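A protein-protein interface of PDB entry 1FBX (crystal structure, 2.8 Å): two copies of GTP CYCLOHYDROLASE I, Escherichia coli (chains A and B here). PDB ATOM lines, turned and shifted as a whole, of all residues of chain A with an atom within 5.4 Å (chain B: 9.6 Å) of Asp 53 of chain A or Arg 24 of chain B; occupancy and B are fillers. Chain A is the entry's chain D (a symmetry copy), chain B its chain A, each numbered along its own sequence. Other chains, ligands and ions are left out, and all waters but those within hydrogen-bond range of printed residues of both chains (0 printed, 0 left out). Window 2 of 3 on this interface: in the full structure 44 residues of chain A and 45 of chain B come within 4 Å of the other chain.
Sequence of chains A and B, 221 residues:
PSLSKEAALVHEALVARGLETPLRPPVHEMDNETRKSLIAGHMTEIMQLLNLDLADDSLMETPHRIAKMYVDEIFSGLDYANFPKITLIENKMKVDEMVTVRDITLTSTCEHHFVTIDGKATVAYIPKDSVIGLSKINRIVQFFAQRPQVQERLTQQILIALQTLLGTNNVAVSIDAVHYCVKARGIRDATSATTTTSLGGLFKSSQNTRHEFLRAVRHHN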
ATOM      1  N   GLN A  48      21.538  28.375  10.837  1.00  0.00           N
ATOM      2  CA  GLN A  48      20.379  27.563  10.449  1.00  0.00           C
ATOM      3  C   GLN A  48      20.763  26.509   9.410  1.00  0.00           C
ATOM      4  O   GLN A  48      20.231  25.402   9.387  1.00  0.00           O
ATOM      5  CB  GLN A  48      19.256  28.444   9.929  1.00  0.00           C
ATOM      6  CG  GLN A  48      18.744  29.385  10.989  1.00  0.00           C
ATOM      7  CD  GLN A  48      17.362  29.921  10.683  1.00  0.00           C
ATOM      8  OE1 GLN A  48      17.023  30.157   9.525  1.00  0.00           O
ATOM      9  NE2 GLN A  48      16.562  30.135  11.727  1.00  0.00           N
ATOM     10  N   ASN A  51      21.544  23.524  11.112  1.00  0.00           N
ATOM     11  CA  ASN A  51      20.405  22.868  11.730  1.00  0.00           C
ATOM     12  C   ASN A  51      20.337  23.085  13.226  1.00  0.00           C
ATOM     13  O   ASN A  51      19.754  22.290  13.968  1.00  0.00           O
ATOM     14  CB  ASN A  51      20.409  21.366  11.433  1.00  0.00           C
ATOM     15  CG  ASN A  51      20.296  21.064   9.950  1.00  0.00           C
ATOM     16  OD1 ASN A  51      19.598  21.759   9.226  1.00  0.00           O
ATOM     17  ND2 ASN A  51      20.971  20.011   9.495  1.00  0.00           N
ATOM     18  N   LEU A  52      20.936  24.164  13.687  1.00  0.00           N
ATOM     19  CA  LEU A  52      20.871  24.423  15.106  1.00  0.00           C
ATOM     20  C   LEU A  52      19.487  25.017  15.383  1.00  0.00           C
ATOM     21  O   LEU A  52      18.865  25.616  14.503  1.00  0.00           O
ATOM     22  CB  LEU A  52      22.014  25.372  15.525  1.00  0.00           C
ATOM     23  CG  LEU A  52      23.404  24.745  15.322  1.00  0.00           C
ATOM     24  CD1 LEU A  52      24.489  25.787  15.411  1.00  0.00           C
ATOM     25  CD2 LEU A  52      23.597  23.647  16.354  1.00  0.00           C
ATOM     26  N   ASP A  53      18.983  24.812  16.589  1.00  0.00           N
ATOM     27  CA  ASP A  53      17.695  25.359  16.937  1.00  0.00           C
ATOM     28  C   ASP A  53      17.902  26.691  17.641  1.00  0.00           C
ATOM     29  O   ASP A  53      18.153  26.731  18.849  1.00  0.00           O
ATOM     30  CB  ASP A  53      16.937  24.392  17.836  1.00  0.00           C
ATOM     31  CG  ASP A  53      15.652  24.993  18.361  1.00  0.00           C
ATOM     32  OD1 ASP A  53      14.960  25.711  17.591  1.00  0.00           O
ATOM     33  OD2 ASP A  53      15.325  24.752  19.540  1.00  0.00           O
ATOM     34  N   LEU A  54      17.808  27.780  16.879  1.00  0.00           N
ATOM     35  CA  LEU A  54      17.995  29.122  17.425  1.00  0.00           C
ATOM     36  C   LEU A  54      16.969  29.494  18.482  1.00  0.00           C
ATOM     37  O   LEU A  54      17.083  30.527  19.145  1.00  0.00           O
ATOM     38  CB  LEU A  54      17.964  30.160  16.315  1.00  0.00           C
ATOM     39  CG  LEU A  54      19.237  30.268  15.495  1.00  0.00           C
ATOM     40  CD1 LEU A  54      19.050  31.359  14.480  1.00  0.00           C
ATOM     41  CD2 LEU A  54      20.423  30.593  16.387  1.00  0.00           C
ATOM     42  N   ALA A  55      15.957  28.658  18.642  1.00  0.00           N
ATOM     43  CA  ALA A  55      14.948  28.923  19.643  1.00  0.00           C
ATOM     44  C   ALA A  55      15.535  28.726  21.028  1.00  0.00           C
ATOM     45  O   ALA A  55      15.042  29.301  21.987  1.00  0.00           O
ATOM     46  CB  ALA A  55      13.797  27.997  19.452  1.00  0.00           C
ATOM     47  N   ASP A  56      16.597  27.925  21.125  1.00  0.00           N
ATOM     48  CA  ASP A  56      17.246  27.611  22.402  1.00  0.00           C
ATOM     49  C   ASP A  56      17.732  28.780  23.255  1.00  0.00           C
ATOM     50  O   ASP A  56      18.311  29.734  22.750  1.00  0.00           O
ATOM     51  CB  ASP A  56      18.418  26.664  22.179  1.00  0.00           C
ATOM     52  CG  ASP A  56      18.941  26.095  23.486  1.00  0.00           C
ATOM     53  OD1 ASP A  56      18.156  25.404  24.180  1.00  0.00           O
ATOM     54  OD2 ASP A  56      20.125  26.343  23.821  1.00  0.00           O
ATOM     55  N   LEU A  59      21.434  29.339  22.467  1.00  0.00           N
ATOM     56  CA  LEU A  59      21.820  29.685  21.099  1.00  0.00           C
ATOM     57  C   LEU A  59      21.283  31.012  20.551  1.00  0.00           C
ATOM     58  O   LEU A  59      21.950  31.703  19.796  1.00  0.00           O
ATOM     59  CB  LEU A  59      21.439  28.535  20.159  1.00  0.00           C
ATOM     60  CG  LEU A  59      22.234  27.236  20.305  1.00  0.00           C
ATOM     61  CD1 LEU A  59      21.713  26.223  19.325  1.00  0.00           C
ATOM     62  CD2 LEU A  59      23.702  27.485  20.040  1.00  0.00           C
ATOM     63  N   HIS B  11      22.059   8.409  19.945  1.00  0.00           N
ATOM     64  CA  HIS B  11      21.165   9.517  19.647  1.00  0.00           C
ATOM     65  C   HIS B  11      19.859   9.469  20.440  1.00  0.00           C
ATOM     66  O   HIS B  11      19.473  10.454  21.070  1.00  0.00           O
ATOM     67  CB  HIS B  11      20.854   9.558  18.154  1.00  0.00           C
ATOM     68  CG  HIS B  11      19.943  10.685  17.770  1.00  0.00           C
ATOM     69  ND1 HIS B  11      19.534  11.647  18.659  1.00  0.00           N
ATOM     70  CD2 HIS B  11      19.407  11.023  16.574  1.00  0.00           C
ATOM     71  CE1 HIS B  11      18.784  12.542  18.034  1.00  0.00           C
ATOM     72  NE2 HIS B  11      18.695  12.186  16.770  1.00  0.00           N
ATOM     73  N   GLU B  20      20.469  16.189  23.996  1.00  0.00           N
ATOM     74  CA  GLU B  20      21.012  16.300  22.652  1.00  0.00           C
ATOM     75  C   GLU B  20      21.321  17.750  22.347  1.00  0.00           C
ATOM     76  O   GLU B  20      20.749  18.660  22.934  1.00  0.00           O
ATOM     77  CB  GLU B  20      20.036  15.775  21.600  1.00  0.00           C
ATOM     78  CG  GLU B  20      20.513  14.517  20.905  1.00  0.00           C
ATOM     79  CD  GLU B  20      21.735  14.721  20.034  1.00  0.00           C
ATOM     80  OE1 GLU B  20      22.557  15.619  20.305  1.00  0.00           O
ATOM     81  OE2 GLU B  20      21.883  13.953  19.072  1.00  0.00           O
ATOM     82  N   THR B  21      22.245  17.972  21.435  1.00  0.00           N
ATOM     83  CA  THR B  21      22.551  19.328  21.054  1.00  0.00           C
ATOM     84  C   THR B  21      21.270  19.849  20.425  1.00  0.00           C
ATOM     85  O   THR B  21      20.611  19.131  19.681  1.00  0.00           O
ATOM     86  CB  THR B  21      23.673  19.343  20.031  1.00  0.00           C
ATOM     87  OG1 THR B  21      24.908  19.023  20.691  1.00  0.00           O
ATOM     88  CG2 THR B  21      23.758  20.699  19.353  1.00  0.00           C
ATOM     89  N   PRO B  22      20.870  21.084  20.747  1.00  0.00           N
ATOM     90  CA  PRO B  22      19.646  21.668  20.178  1.00  0.00           C
ATOM     91  C   PRO B  22      19.648  21.730  18.646  1.00  0.00           C
ATOM     92  O   PRO B  22      20.236  22.628  18.047  1.00  0.00           O
ATOM     93  CB  PRO B  22      19.608  23.053  20.808  1.00  0.00           C
ATOM     94  CG  PRO B  22      20.173  22.780  22.163  1.00  0.00           C
ATOM     95  CD  PRO B  22      21.373  21.911  21.851  1.00  0.00           C
ATOM     96  N   LEU B  23      18.979  20.762  18.024  1.00  0.00           N
ATOM     97  CA  LEU B  23      18.888  20.690  16.572  1.00  0.00           C
ATOM     98  C   LEU B  23      17.469  20.802  16.028  1.00  0.00           C
ATOM     99  O   LEU B  23      16.505  20.410  16.688  1.00  0.00           O
ATOM    100  CB  LEU B  23      19.483  19.379  16.086  1.00  0.00           C
ATOM    101  CG  LEU B  23      20.970  19.306  15.807  1.00  0.00           C
ATOM    102  CD1 LEU B  23      21.637  20.587  16.259  1.00  0.00           C
ATOM    103  CD2 LEU B  23      21.532  18.085  16.498  1.00  0.00           C
ATOM    104  N   ARG B  24      17.358  21.344  14.815  1.00  0.00           N
ATOM    105  CA  ARG B  24      16.073  21.484  14.127  1.00  0.00           C
ATOM    106  C   ARG B  24      16.045  20.481  12.997  1.00  0.00           C
ATOM    107  O   ARG B  24      17.064  20.243  12.350  1.00  0.00           O
ATOM    108  CB  ARG B  24      15.908  22.861  13.499  1.00  0.00           C
ATOM    109  CG  ARG B  24      15.317  23.906  14.386  1.00  0.00           C
ATOM    110  CD  ARG B  24      15.450  25.241  13.684  1.00  0.00           C
ATOM    111  NE  ARG B  24      15.381  26.368  14.610  1.00  0.00           N
ATOM    112  CZ  ARG B  24      15.766  27.600  14.300  1.00  0.00           C
ATOM    113  NH1 ARG B  24      16.247  27.854  13.087  1.00  0.00           N
ATOM    114  NH2 ARG B  24      15.675  28.569  15.200  1.00  0.00           N
ATOM    115  N   PRO B  25      14.870  19.887  12.735  1.00  0.00           N
ATOM    116  CA  PRO B  25      14.784  18.910  11.651  1.00  0.00           C
ATOM    117  C   PRO B  25      15.354  19.553  10.393  1.00  0.00           C
ATOM    118  O   PRO B  25      15.099  20.733  10.104  1.00  0.00           O
ATOM    119  CB  PRO B  25      13.282  18.645  11.542  1.00  0.00           C
ATOM    120  CG  PRO B  25      12.792  18.878  12.937  1.00  0.00           C
ATOM    121  CD  PRO B  25      13.543  20.126  13.332  1.00  0.00           C
ATOM    122  N   PRO B  26      16.154  18.791   9.637  1.00  0.00           N
ATOM    123  CA  PRO B  26      16.722  19.373   8.420  1.00  0.00           C
ATOM    124  C   PRO B  26      15.640  20.097   7.630  1.00  0.00           C
ATOM    125  O   PRO B  26      15.880  21.162   7.079  1.00  0.00           O
ATOM    126  CB  PRO B  26      17.279  18.152   7.691  1.00  0.00           C
ATOM    127  CG  PRO B  26      17.721  17.250   8.839  1.00  0.00           C
ATOM    128  CD  PRO B  26      16.549  17.376   9.799  1.00  0.00           C
ATOM    129  N   ARG B  35      24.650  23.598   0.970  1.00  0.00           N
ATOM    130  CA  ARG B  35      24.836  24.142   2.310  1.00  0.00           C
ATOM    131  C   ARG B  35      26.164  24.885   2.404  1.00  0.00           C
ATOM    132  O   ARG B  35      26.227  26.063   2.771  1.00  0.00           O
ATOM    133  CB  ARG B  35      24.820  23.032   3.346  1.00  0.00           C
ATOM    134  CG  ARG B  35      23.469  22.440   3.557  1.00  0.00           C
ATOM    135  CD  ARG B  35      23.322  21.985   4.991  1.00  0.00           C
ATOM    136  NE  ARG B  35      24.258  20.923   5.320  1.00  0.00           N
ATOM    137  CZ  ARG B  35      24.548  20.549   6.559  1.00  0.00           C
ATOM    138  NH1 ARG B  35      23.980  21.159   7.592  1.00  0.00           N
ATOM    139  NH2 ARG B  35      25.395  19.552   6.764  1.00  0.00           N
ATOM    140  N   LEU B  78      27.643  17.092  14.379  1.00  0.00           N
ATOM    141  CA  LEU B  78      26.233  17.464  14.409  1.00  0.00           C
ATOM    142  C   LEU B  78      25.454  16.463  13.575  1.00  0.00           C
ATOM    143  O   LEU B  78      24.246  16.334  13.740  1.00  0.00           O
ATOM    144  CB  LEU B  78      26.015  18.870  13.858  1.00  0.00           C
ATOM    145  CG  LEU B  78      26.383  20.011  14.799  1.00  0.00           C
ATOM    146  CD1 LEU B  78      26.227  21.349  14.099  1.00  0.00           C
ATOM    147  CD2 LEU B  78      25.508  19.934  16.027  1.00  0.00           C
ATOM    148  N   GLU B 111      29.707  27.598  22.002  1.00  0.00           N
ATOM    149  CA  GLU B 111      28.510  27.927  21.243  1.00  0.00           C
ATOM    150  C   GLU B 111      28.022  29.373  21.435  1.00  0.00           C
ATOM    151  O   GLU B 111      27.029  29.792  20.804  1.00  0.00           O
ATOM    152  CB  GLU B 111      27.381  26.945  21.598  1.00  0.00           C
ATOM    153  CG  GLU B 111      26.704  27.219  22.898  1.00  0.00           C
ATOM    154  CD  GLU B 111      25.658  26.171  23.207  1.00  0.00           C
ATOM    155  OE1 GLU B 111      25.863  25.008  22.776  1.00  0.00           O
ATOM    156  OE2 GLU B 111      24.643  26.479  23.884  1.00  0.00           O
ATOM    157  N   PRO B 148      29.059  22.851  18.384  1.00  0.00           N
ATOM    158  CA  PRO B 148      29.120  24.101  19.143  1.00  0.00           C
ATOM    159  C   PRO B 148      28.678  23.604  20.529  1.00  0.00           C
ATOM    160  O   PRO B 148      27.530  23.200  20.709  1.00  0.00           O
ATOM    161  CB  PRO B 148      28.058  24.957  18.469  1.00  0.00           C
ATOM    162  CG  PRO B 148      28.045  24.446  17.078  1.00  0.00           C
ATOM    163  CD  PRO B 148      28.093  22.963  17.284  1.00  0.00           C
ATOM    164  N   ARG B 153      27.408  20.408  28.949  1.00  0.00           N
ATOM    165  CA  ARG B 153      26.638  19.450  28.166  1.00  0.00           C
ATOM    166  C   ARG B 153      27.509  18.392  27.518  1.00  0.00           C
ATOM    167  O   ARG B 153      27.145  17.216  27.477  1.00  0.00           O
ATOM    168  CB  ARG B 153      25.823  20.158  27.091  1.00  0.00           C
ATOM    169  CG  ARG B 153      24.839  19.242  26.369  1.00  0.00           C
ATOM    170  CD  ARG B 153      24.232  19.931  25.145  1.00  0.00           C
ATOM    171  NE  ARG B 153      23.362  21.049  25.509  1.00  0.00           N
ATOM    172  CZ  ARG B 153      23.548  22.307  25.112  1.00  0.00           C
ATOM    173  NH1 ARG B 153      24.580  22.621  24.330  1.00  0.00           N
ATOM    174  NH2 ARG B 153      22.700  23.257  25.500  1.00  0.00           N
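The backbone carbonyl oxygen (O) of Pro 22 of chain B is in hydrogen-bond range of the backbone NH (N) of Asp 53 of chain A, 2.9 Å away.
NH1 of Arg 24 of chain B lies close to NE2 of Gln 48 of chain A (2.7 Å).
The backbone carbonyl oxygen of Asn 51 of chain A sits at hydrogen-bond distance from the backbone NH of Arg 24 of chain B.
OD1 of Asp 53 of chain A lies within salt-bridge range of NE of Arg 24 of chain B (3.1 Å).
NH2 of Arg 24 of chain B sits close to N of Leu 54 of chain A, at 2.8 Å.
N of Ala 55 of chain A lies close to NH2 of Arg 24 of chain B (3.5 Å).
The side-chain carboxylate of Glu 111 of chain B lies within salt-bridge range of the guanidinium group of Arg 153 of chain B (3.1 Å).
N of Ala 55 of chain A lies close to OD1 of Asp 53 of chain A.
Among the printed residues, pairs that only touch across the chains: Asn 51 of chain A with Leu 23 of chain B (3.2 Å), Leu 52 of chain A with Pro 22 of chain B (3.5 Å), Leu 52 of chain A with Arg 24 of chain B (3.5 Å), Leu 52 of chain A with Leu 23 of chain B (3.6 Å), Asn 51 of chain A with Arg 35 of chain B (3.7 Å), Asp 56 of chain A with Pro 22 of chain B (3.8 Å), Asn 51 of chain A with Pro 26 of chain B (3.8 Å) and Leu 59 of chain A with Glu 111 of chain B (3.9 Å).
Of chain B, only Pro 22 (2.9 Å) and Arg 24 (3.1 Å) come within 4 Å of Asp 53 of chain A.
Of the printed residues of chain B, Ala 55 of chain A touches Arg 24.
Of chain B, only Pro 22 comes within 4 Å of Asp 56 of chain A.
Printed residues of chain B within 4 Å of Leu 59 of chain A: Glu 111.
Of the printed residues of chain A, Leu 23 of chain B touches Asn 51 and Leu 52.
Printed residues of chain A within 4 Å of Arg 24 of chain B: Gln 48 (2.7 Å), Asn 51 (2.7 Å), Leu 52 (3.5 Å), Asp 53 (3.1 Å), Leu 54 (2.8 Å) and Ala 55 (3.5 Å).
Pro 25 of chain B touches none of the printed residues of chain A.
Of the printed residues of chain A, Pro 26 of chain B touches Asn 51 (3.8 Å).
Leu 78 of chain B touches none of the printed residues of chain A.
Hydrophobic or aromatic side chains of chain A that line the printed part of chain B: Leu 52, Leu 54 and Leu 59.
Hydrophobic or aromatic side chains of chain B that line the printed part of chain A: Pro 22 and Leu 23.
No position is printed for both chains.
Of the 14 pairs that touch across the chains among the printed residues, none has its exchanged pair printed and touching as well.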
